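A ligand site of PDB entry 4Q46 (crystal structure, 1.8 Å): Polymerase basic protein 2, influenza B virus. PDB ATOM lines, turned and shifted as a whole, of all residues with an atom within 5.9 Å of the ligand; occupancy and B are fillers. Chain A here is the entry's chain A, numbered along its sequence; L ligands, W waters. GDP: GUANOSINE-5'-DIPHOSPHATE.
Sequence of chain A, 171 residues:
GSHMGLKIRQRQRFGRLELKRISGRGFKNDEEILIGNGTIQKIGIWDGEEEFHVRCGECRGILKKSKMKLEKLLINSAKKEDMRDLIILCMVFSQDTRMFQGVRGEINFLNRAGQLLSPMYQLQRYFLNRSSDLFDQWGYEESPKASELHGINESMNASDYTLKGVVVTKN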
ATOM      1  N   GLN A  12     -10.313 -17.154 -27.137  1.00  0.00           N
ATOM      2  CA  GLN A  12     -10.886 -18.244 -27.826  1.00  0.00           C
ATOM      3  C   GLN A  12     -11.936 -17.830 -28.803  1.00  0.00           C
ATOM      4  O   GLN A  12     -12.431 -16.701 -28.718  1.00  0.00           O
ATOM      5  CB  GLN A  12     -11.384 -19.347 -26.850  1.00  0.00           C
ATOM      6  CG  GLN A  12     -12.773 -19.176 -26.172  1.00  0.00           C
ATOM      7  CD  GLN A  12     -12.920 -19.899 -24.748  1.00  0.00           C
ATOM      8  OE1 GLN A  12     -13.400 -21.020 -24.610  1.00  0.00           O
ATOM      9  NE2 GLN A  12     -12.493 -19.201 -23.709  1.00  0.00           N
ATOM     10  N   ARG A  13     -12.348 -18.725 -29.712  1.00  0.00           N
ATOM     11  CA  ARG A  13     -13.396 -18.343 -30.662  1.00  0.00           C
ATOM     12  C   ARG A  13     -14.619 -19.217 -30.551  1.00  0.00           C
ATOM     13  O   ARG A  13     -14.480 -20.403 -30.246  1.00  0.00           O
ATOM     14  CB  ARG A  13     -12.873 -18.398 -32.120  1.00  0.00           C
ATOM     15  CG  ARG A  13     -11.668 -17.463 -32.403  1.00  0.00           C
ATOM     16  CD  ARG A  13     -11.987 -15.995 -32.140  1.00  0.00           C
ATOM     17  NE  ARG A  13     -13.059 -15.527 -33.023  1.00  0.00           N
ATOM     18  CZ  ARG A  13     -12.951 -14.592 -33.982  1.00  0.00           C
ATOM     19  NH1 ARG A  13     -11.793 -13.968 -34.264  1.00  0.00           N
ATOM     20  NH2 ARG A  13     -14.009 -14.261 -34.670  1.00  0.00           N
ATOM     21  N   PHE A  14     -15.828 -18.622 -30.757  1.00  0.00           N
ATOM     22  CA  PHE A  14     -17.060 -19.366 -31.088  1.00  0.00           C
ATOM     23  C   PHE A  14     -17.490 -18.765 -32.440  1.00  0.00           C
ATOM     24  O   PHE A  14     -18.325 -17.862 -32.490  1.00  0.00           O
ATOM     25  CB  PHE A  14     -18.156 -19.083 -30.018  1.00  0.00           C
ATOM     26  CG  PHE A  14     -19.548 -19.658 -30.354  1.00  0.00           C
ATOM     27  CD1 PHE A  14     -19.715 -20.926 -30.918  1.00  0.00           C
ATOM     28  CD2 PHE A  14     -20.703 -18.882 -30.119  1.00  0.00           C
ATOM     29  CE1 PHE A  14     -21.039 -21.424 -31.209  1.00  0.00           C
ATOM     30  CE2 PHE A  14     -22.041 -19.366 -30.433  1.00  0.00           C
ATOM     31  CZ  PHE A  14     -22.178 -20.644 -30.959  1.00  0.00           C
ATOM     32  N   LEU A  19     -13.888 -14.618 -27.413  1.00  0.00           N
ATOM     33  CA  LEU A  19     -14.115 -14.504 -25.966  1.00  0.00           C
ATOM     34  C   LEU A  19     -12.824 -14.729 -25.226  1.00  0.00           C
ATOM     35  O   LEU A  19     -11.900 -15.386 -25.731  1.00  0.00           O
ATOM     36  CB  LEU A  19     -15.080 -15.613 -25.465  1.00  0.00           C
ATOM     37  CG  LEU A  19     -16.398 -15.792 -26.189  1.00  0.00           C
ATOM     38  CD1 LEU A  19     -16.318 -16.983 -27.200  1.00  0.00           C
ATOM     39  CD2 LEU A  19     -17.442 -16.110 -25.078  1.00  0.00           C
ATOM     40  N   ARG A  21     -12.179 -15.513 -21.003  1.00  0.00           N
ATOM     41  CA  ARG A  21     -12.799 -15.615 -19.655  1.00  0.00           C
ATOM     42  C   ARG A  21     -12.276 -14.584 -18.680  1.00  0.00           C
ATOM     43  O   ARG A  21     -11.030 -14.304 -18.589  1.00  0.00           O
ATOM     44  CB  ARG A  21     -12.605 -17.017 -19.047  1.00  0.00           C
ATOM     45  CG  ARG A  21     -13.362 -17.178 -17.695  1.00  0.00           C
ATOM     46  CD  ARG A  21     -13.111 -18.559 -17.101  1.00  0.00           C
ATOM     47  NE  ARG A  21     -13.441 -19.596 -18.090  1.00  0.00           N
ATOM     48  CZ  ARG A  21     -14.687 -20.036 -18.301  1.00  0.00           C
ATOM     49  NH1 ARG A  21     -15.690 -19.529 -17.604  1.00  0.00           N
ATOM     50  NH2 ARG A  21     -14.910 -20.933 -19.239  1.00  0.00           N
ATOM     51  N   GLY A  26     -18.004 -23.004 -16.138  1.00  0.00           N
ATOM     52  CA  GLY A  26     -19.174 -23.759 -16.559  1.00  0.00           C
ATOM     53  C   GLY A  26     -18.842 -25.249 -16.635  1.00  0.00           C
ATOM     54  O   GLY A  26     -17.689 -25.665 -16.923  1.00  0.00           O
ATOM     55  N   LYS A  28     -20.396 -28.698 -18.541  1.00  0.00           N
ATOM     56  CA  LYS A  28     -21.288 -29.029 -19.663  1.00  0.00           C
ATOM     57  C   LYS A  28     -21.922 -30.421 -19.485  1.00  0.00           C
ATOM     58  O   LYS A  28     -21.217 -31.415 -19.091  1.00  0.00           O
ATOM     59  CB  LYS A  28     -20.479 -28.913 -20.977  1.00  0.00           C
ATOM     60  CG  LYS A  28     -21.349 -29.269 -22.230  1.00  0.00           C
ATOM     61  CD  LYS A  28     -20.572 -28.966 -23.526  1.00  0.00           C
ATOM     62  CE  LYS A  28     -19.333 -29.784 -23.657  1.00  0.00           C
ATOM     63  NZ  LYS A  28     -19.837 -31.190 -23.786  1.00  0.00           N
ATOM     64  N   ASP A  30     -25.099 -32.962 -21.510  1.00  0.00           N
ATOM     65  CA  ASP A  30     -26.078 -33.087 -22.606  1.00  0.00           C
ATOM     66  C   ASP A  30     -27.502 -33.024 -22.039  1.00  0.00           C
ATOM     67  O   ASP A  30     -27.779 -33.655 -21.000  1.00  0.00           O
ATOM     68  CB  ASP A  30     -25.856 -34.404 -23.363  1.00  0.00           C
ATOM     69  CG  ASP A  30     -24.810 -34.285 -24.530  1.00  0.00           C
ATOM     70  OD1 ASP A  30     -24.298 -33.189 -24.797  1.00  0.00           O
ATOM     71  OD2 ASP A  30     -24.593 -35.286 -25.262  1.00  0.00           O
ATOM     72  N   ILE A  43     -28.243 -31.271 -26.913  1.00  0.00           N
ATOM     73  CA  ILE A  43     -27.191 -30.197 -26.932  1.00  0.00           C
ATOM     74  C   ILE A  43     -26.409 -30.218 -25.638  1.00  0.00           C
ATOM     75  O   ILE A  43     -26.980 -30.431 -24.568  1.00  0.00           O
ATOM     76  CB  ILE A  43     -27.825 -28.797 -27.121  1.00  0.00           C
ATOM     77  CG1 ILE A  43     -28.658 -28.782 -28.418  1.00  0.00           C
ATOM     78  CG2 ILE A  43     -26.714 -27.715 -27.159  1.00  0.00           C
ATOM     79  CD1 ILE A  43     -29.320 -27.522 -28.609  1.00  0.00           C
ATOM     80  N   GLY A  44     -25.078 -30.036 -25.705  1.00  0.00           N
ATOM     81  CA  GLY A  44     -24.366 -29.821 -24.440  1.00  0.00           C
ATOM     82  C   GLY A  44     -24.587 -28.433 -23.854  1.00  0.00           C
ATOM     83  O   GLY A  44     -24.229 -27.399 -24.487  1.00  0.00           O
ATOM     84  N   TRP A  46     -24.183 -25.670 -20.806  1.00  0.00           N
ATOM     85  CA  TRP A  46     -23.255 -25.246 -19.738  1.00  0.00           C
ATOM     86  C   TRP A  46     -24.040 -24.789 -18.507  1.00  0.00           C
ATOM     87  O   TRP A  46     -24.994 -24.023 -18.603  1.00  0.00           O
ATOM     88  CB  TRP A  46     -22.335 -24.151 -20.259  1.00  0.00           C
ATOM     89  CG  TRP A  46     -21.513 -24.661 -21.372  1.00  0.00           C
ATOM     90  CD1 TRP A  46     -21.823 -24.697 -22.725  1.00  0.00           C
ATOM     91  CD2 TRP A  46     -20.204 -25.259 -21.248  1.00  0.00           C
ATOM     92  NE1 TRP A  46     -20.786 -25.283 -23.421  1.00  0.00           N
ATOM     93  CE2 TRP A  46     -19.771 -25.592 -22.538  1.00  0.00           C
ATOM     94  CE3 TRP A  46     -19.324 -25.460 -20.149  1.00  0.00           C
ATOM     95  CZ2 TRP A  46     -18.502 -26.166 -22.783  1.00  0.00           C
ATOM     96  CZ3 TRP A  46     -18.083 -26.055 -20.371  1.00  0.00           C
ATOM     97  CH2 TRP A  46     -17.679 -26.401 -21.699  1.00  0.00           C
ATOM     98  N   GLU A  50     -20.610 -17.605 -15.353  1.00  0.00           N
ATOM     99  CA  GLU A  50     -19.408 -17.300 -16.141  1.00  0.00           C
ATOM    100  C   GLU A  50     -19.428 -15.891 -16.637  1.00  0.00           C
ATOM    101  O   GLU A  50     -20.516 -15.348 -16.985  1.00  0.00           O
ATOM    102  CB  GLU A  50     -19.323 -18.217 -17.381  1.00  0.00           C
ATOM    103  CG  GLU A  50     -19.180 -19.707 -16.968  1.00  0.00           C
ATOM    104  CD  GLU A  50     -19.156 -20.596 -18.184  1.00  0.00           C
ATOM    105  OE1 GLU A  50     -20.219 -21.145 -18.630  1.00  0.00           O
ATOM    106  OE2 GLU A  50     -18.047 -20.739 -18.715  1.00  0.00           O
ATOM    107  N   PHE A  52     -17.263 -13.224 -19.378  1.00  0.00           N
ATOM    108  CA  PHE A  52     -16.246 -13.185 -20.484  1.00  0.00           C
ATOM    109  C   PHE A  52     -16.118 -11.791 -21.050  1.00  0.00           C
ATOM    110  O   PHE A  52     -17.075 -11.033 -21.166  1.00  0.00           O
ATOM    111  CB  PHE A  52     -16.670 -14.095 -21.713  1.00  0.00           C
ATOM    112  CG  PHE A  52     -16.782 -15.550 -21.389  1.00  0.00           C
ATOM    113  CD1 PHE A  52     -15.668 -16.399 -21.524  1.00  0.00           C
ATOM    114  CD2 PHE A  52     -18.008 -16.094 -20.937  1.00  0.00           C
ATOM    115  CE1 PHE A  52     -15.777 -17.777 -21.248  1.00  0.00           C
ATOM    116  CE2 PHE A  52     -18.085 -17.430 -20.633  1.00  0.00           C
ATOM    117  CZ  PHE A  52     -17.005 -18.275 -20.793  1.00  0.00           C
ATOM    118  N   LYS A  65     -23.239 -14.780 -17.968  1.00  0.00           N
ATOM    119  CA  LYS A  65     -24.227 -15.798 -18.288  1.00  0.00           C
ATOM    120  C   LYS A  65     -24.401 -16.723 -17.091  1.00  0.00           C
ATOM    121  O   LYS A  65     -23.534 -16.778 -16.190  1.00  0.00           O
ATOM    122  CB  LYS A  65     -23.876 -16.645 -19.575  1.00  0.00           C
ATOM    123  CG  LYS A  65     -22.857 -17.772 -19.233  1.00  0.00           C
ATOM    124  CD  LYS A  65     -22.593 -18.802 -20.304  1.00  0.00           C
ATOM    125  CE  LYS A  65     -23.793 -19.488 -20.801  1.00  0.00           C
ATOM    126  NZ  LYS A  65     -24.278 -20.457 -19.814  1.00  0.00           N
ATOM    127  N   PHE A  93     -24.463 -17.854 -27.587  1.00  0.00           N
ATOM    128  CA  PHE A  93     -23.400 -18.402 -26.739  1.00  0.00           C
ATOM    129  C   PHE A  93     -23.961 -18.594 -25.307  1.00  0.00           C
ATOM    130  O   PHE A  93     -23.601 -19.568 -24.624  1.00  0.00           O
ATOM    131  CB  PHE A  93     -22.219 -17.452 -26.658  1.00  0.00           C
ATOM    132  CG  PHE A  93     -21.102 -18.003 -25.779  1.00  0.00           C
ATOM    133  CD1 PHE A  93     -20.238 -18.998 -26.299  1.00  0.00           C
ATOM    134  CD2 PHE A  93     -20.982 -17.603 -24.417  1.00  0.00           C
ATOM    135  CE1 PHE A  93     -19.253 -19.568 -25.501  1.00  0.00           C
ATOM    136  CE2 PHE A  93     -19.996 -18.208 -23.649  1.00  0.00           C
ATOM    137  CZ  PHE A  93     -19.131 -19.156 -24.212  1.00  0.00           C
ATOM    138  N   GLN A  95     -26.774 -19.629 -24.558  1.00  0.00           N
ATOM    139  CA  GLN A  95     -27.759 -20.740 -24.581  1.00  0.00           C
ATOM    140  C   GLN A  95     -29.047 -20.309 -23.908  1.00  0.00           C
ATOM    141  O   GLN A  95     -29.724 -21.138 -23.313  1.00  0.00           O
ATOM    142  CB  GLN A  95     -27.228 -22.047 -23.916  1.00  0.00           C
ATOM    143  CG  GLN A  95     -25.902 -22.480 -24.610  1.00  0.00           C
ATOM    144  CD  GLN A  95     -25.324 -23.747 -23.994  1.00  0.00           C
ATOM    145  OE1 GLN A  95     -25.145 -23.854 -22.781  1.00  0.00           O
ATOM    146  NE2 GLN A  95     -24.917 -24.689 -24.897  1.00  0.00           N
ATOM    147  N   SER A 118     -22.221 -29.359 -35.512  1.00  0.00           N
ATOM    148  CA  SER A 118     -22.402 -28.937 -34.099  1.00  0.00           C
ATOM    149  C   SER A 118     -23.724 -28.163 -33.964  1.00  0.00           C
ATOM    150  O   SER A 118     -23.898 -27.208 -34.670  1.00  0.00           O
ATOM    151  CB  SER A 118     -21.231 -28.017 -33.755  1.00  0.00           C
ATOM    152  OG  SER A 118     -21.499 -27.109 -32.663  1.00  0.00           O
ATOM    153  N   PRO A 119     -24.631 -28.535 -33.048  1.00  0.00           N
ATOM    154  CA  PRO A 119     -25.853 -27.760 -32.834  1.00  0.00           C
ATOM    155  C   PRO A 119     -25.559 -26.293 -32.515  1.00  0.00           C
ATOM    156  O   PRO A 119     -26.275 -25.416 -33.031  1.00  0.00           O
ATOM    157  CB  PRO A 119     -26.515 -28.457 -31.640  1.00  0.00           C
ATOM    158  CG  PRO A 119     -26.095 -29.976 -31.789  1.00  0.00           C
ATOM    159  CD  PRO A 119     -24.634 -29.832 -32.323  1.00  0.00           C
ATOM    160  N   MET A 120     -24.601 -25.985 -31.660  1.00  0.00           N
ATOM    161  CA  MET A 120     -24.375 -24.573 -31.258  1.00  0.00           C
ATOM    162  C   MET A 120     -23.903 -23.749 -32.459  1.00  0.00           C
ATOM    163  O   MET A 120     -24.328 -22.605 -32.656  1.00  0.00           O
ATOM    164  CB  MET A 120     -23.348 -24.435 -30.117  1.00  0.00           C
ATOM    165  CG  MET A 120     -23.984 -24.923 -28.758  1.00  0.00           C
ATOM    166  SD  MET A 120     -25.473 -23.935 -28.317  1.00  0.00           S
ATOM    167  CE  MET A 120     -24.619 -22.492 -28.008  1.00  0.00           C
ATOM    168  N   TYR A 121     -22.986 -24.336 -33.240  1.00  0.00           N
ATOM    169  CA  TYR A 121     -22.513 -23.594 -34.403  1.00  0.00           C
ATOM    170  C   TYR A 121     -23.666 -23.483 -35.402  1.00  0.00           C
ATOM    171  O   TYR A 121     -23.735 -22.440 -36.078  1.00  0.00           O
ATOM    172  CB  TYR A 121     -21.282 -24.291 -35.076  1.00  0.00           C
ATOM    173  CG  TYR A 121     -20.052 -24.059 -34.279  1.00  0.00           C
ATOM    174  CD1 TYR A 121     -19.756 -24.848 -33.149  1.00  0.00           C
ATOM    175  CD2 TYR A 121     -19.244 -22.991 -34.583  1.00  0.00           C
ATOM    176  CE1 TYR A 121     -18.642 -24.603 -32.351  1.00  0.00           C
ATOM    177  CE2 TYR A 121     -18.127 -22.718 -33.796  1.00  0.00           C
ATOM    178  CZ  TYR A 121     -17.835 -23.515 -32.687  1.00  0.00           C
ATOM    179  OH  TYR A 121     -16.724 -23.199 -31.981  1.00  0.00           O
HETATM  180  PB  GDP L   1     -20.169 -30.442 -27.934  1.00  0.00           P
HETATM  181  O1B GDP L   1     -20.915 -31.238 -28.954  1.00  0.00           O
HETATM  182  O2B GDP L   1     -19.048 -31.271 -27.374  1.00  0.00           O
HETATM  183  O3B GDP L   1     -21.142 -29.965 -26.936  1.00  0.00           O
HETATM  184  O3A GDP L   1     -19.289 -29.335 -28.693  1.00  0.00           O
HETATM  185  PA  GDP L   1     -19.616 -28.190 -29.686  1.00  0.00           P
HETATM  186  O1A GDP L   1     -20.691 -28.468 -30.732  1.00  0.00           O
HETATM  187  O2A GDP L   1     -18.315 -27.692 -30.173  1.00  0.00           O
HETATM  188  O5' GDP L   1     -20.191 -26.979 -28.837  1.00  0.00           O
HETATM  189  C5' GDP L   1     -19.500 -26.473 -27.690  1.00  0.00           C
HETATM  190  C4' GDP L   1     -20.149 -25.105 -27.340  1.00  0.00           C
HETATM  191  O4' GDP L   1     -19.625 -24.741 -26.057  1.00  0.00           O
HETATM  192  C3' GDP L   1     -19.708 -23.997 -28.268  1.00  0.00           C
HETATM  193  O3' GDP L   1     -20.855 -23.080 -28.394  1.00  0.00           O
HETATM  194  C2' GDP L   1     -18.473 -23.392 -27.515  1.00  0.00           C
HETATM  195  O2' GDP L   1     -18.277 -22.019 -27.830  1.00  0.00           O
HETATM  196  C1' GDP L   1     -19.050 -23.438 -26.076  1.00  0.00           C
HETATM  197  N9  GDP L   1     -17.994 -23.460 -25.047  1.00  0.00           N
HETATM  198  C8  GDP L   1     -16.717 -24.012 -25.057  1.00  0.00           C
HETATM  199  N7  GDP L   1     -16.167 -23.798 -23.811  1.00  0.00           N
HETATM  200  C5  GDP L   1     -17.084 -23.156 -23.032  1.00  0.00           C
HETATM  201  C6  GDP L   1     -17.127 -22.697 -21.625  1.00  0.00           C
HETATM  202  O6  GDP L   1     -16.099 -22.874 -20.890  1.00  0.00           O
HETATM  203  N1  GDP L   1     -18.259 -22.121 -21.185  1.00  0.00           N
HETATM  204  C2  GDP L   1     -19.365 -21.928 -21.976  1.00  0.00           C
HETATM  205  N2  GDP L   1     -20.479 -21.326 -21.497  1.00  0.00           N
HETATM  206  N3  GDP L   1     -19.392 -22.321 -23.299  1.00  0.00           N
HETATM  207  C4  GDP L   1     -18.270 -22.947 -23.834  1.00  0.00           C
HETATM  208  O   HOH W   1     -22.702 -27.588 -26.768  1.00  0.00           O
HETATM  209  O   HOH W   2     -22.137 -21.731 -24.185  1.00  0.00           O
HETATM  210  O   HOH W   3     -23.748 -30.280 -28.221  1.00  0.00           O
HETATM  211  O   HOH W   4     -17.381 -32.045 -29.787  1.00  0.00           O
HETATM  212  O   HOH W   5     -13.301 -22.853 -21.488  1.00  0.00           O
HETATM  213  O   HOH W   6     -15.471 -26.569 -27.076  1.00  0.00           O
HETATM  214  O   HOH W   7     -15.949 -29.360 -28.456  1.00  0.00           O
HETATM  215  O   HOH W   8     -16.059 -23.671 -18.278  1.00  0.00           O
HETATM  216  O   HOH W   9     -22.044 -32.431 -25.524  1.00  0.00           O
HETATM  217  O   HOH W  10     -23.246 -27.921 -29.787  1.00  0.00           O
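N of Met 120 sits close to OG of Ser 118 (3.4 Å).
The backbone NH (N) of Tyr 121 lies close to the side-chain hydroxyl (OG) of Ser 118, 3.2 Å away.
NH1 of Arg 21 lies within salt-bridge range of OE2 of Glu 50, 2.9 Å away.
The backbone carbonyl oxygen (O) of Glu 50 is in hydrogen-bond range of the backbone NH (N) of Lys 65.
The backbone NH (N) of Gly 26 lies close to the side-chain carboxylate (OE2) of Glu 50 (3.4 Å).
N of Trp 46 lies within hydrogen-bond range of OE1 of Gln 95.
The side-chain sulfur (SD) of Met 120 sits at hydrogen-bond distance from the side-chain amide nitrogen (NE2) of Gln 95 (3.5 Å).
Water W8 lies within hydrogen-bond range of an oxygen (O6) of the ligand (2.7 Å), the backbone carbonyl oxygen (O) of Gly 26 (2.9 Å) and the guanidinium group (NH2) of Arg 21 (3.1 Å).
Water W1 bridges O of Gly 44 (2.8 Å) and O3B of the ligand (2.8 Å).
Water W5 lies within hydrogen-bond range of an oxygen (O6) of the ligand and the guanidinium group (NH2) of Arg 21.
Water W3 lies within hydrogen-bond range of N of Gly 44 and O3B of the ligand.
Water W2 lies within hydrogen-bond range of the backbone carbonyl oxygen (O) of Phe 93 (2.6 Å) and a nitrogen (N3) of the ligand (2.9 Å).
Water W9 lies within hydrogen-bond range of OD1 of Asp 30, O3B of the ligand and NZ of Lys 28.
Phe 14 touches the ligand.
Lys 65 touches the ligand.
Phe 93 touches the ligand.
CB of Met 120 touches O3' of the ligand, at 3.3 Å.
Tyr 121 touches the ligand.
Within 4 Å of the ligand: Phe 14, Arg 21, Lys 28, Trp 46, Glu 50, Lys 65, Phe 93, Ser 118, Met 120 and Tyr 121.
The nearest printed residue that does not touch the ligand is Gln 12 (4.001 Å).
The side-chain hydroxyl (OG) of Ser 118 is in hydrogen-bond range of an oxygen (O1A) of the ligand.
An oxygen (O6) of the ligand lies within hydrogen-bond range of the guanidinium group (NH2) of Arg 21 (2.8 Å).
The side-chain carboxylate (OE2) of Glu 50 sits at hydrogen-bond distance from a nitrogen (N1) of the ligand (2.8 Å).
The indole nitrogen (NE1) of Trp 46 sits at hydrogen-bond distance from an oxygen (O4') of the ligand (2.9 Å).
NZ of Lys 28 lies within salt-bridge range of O3B of the ligand (3.6 Å).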
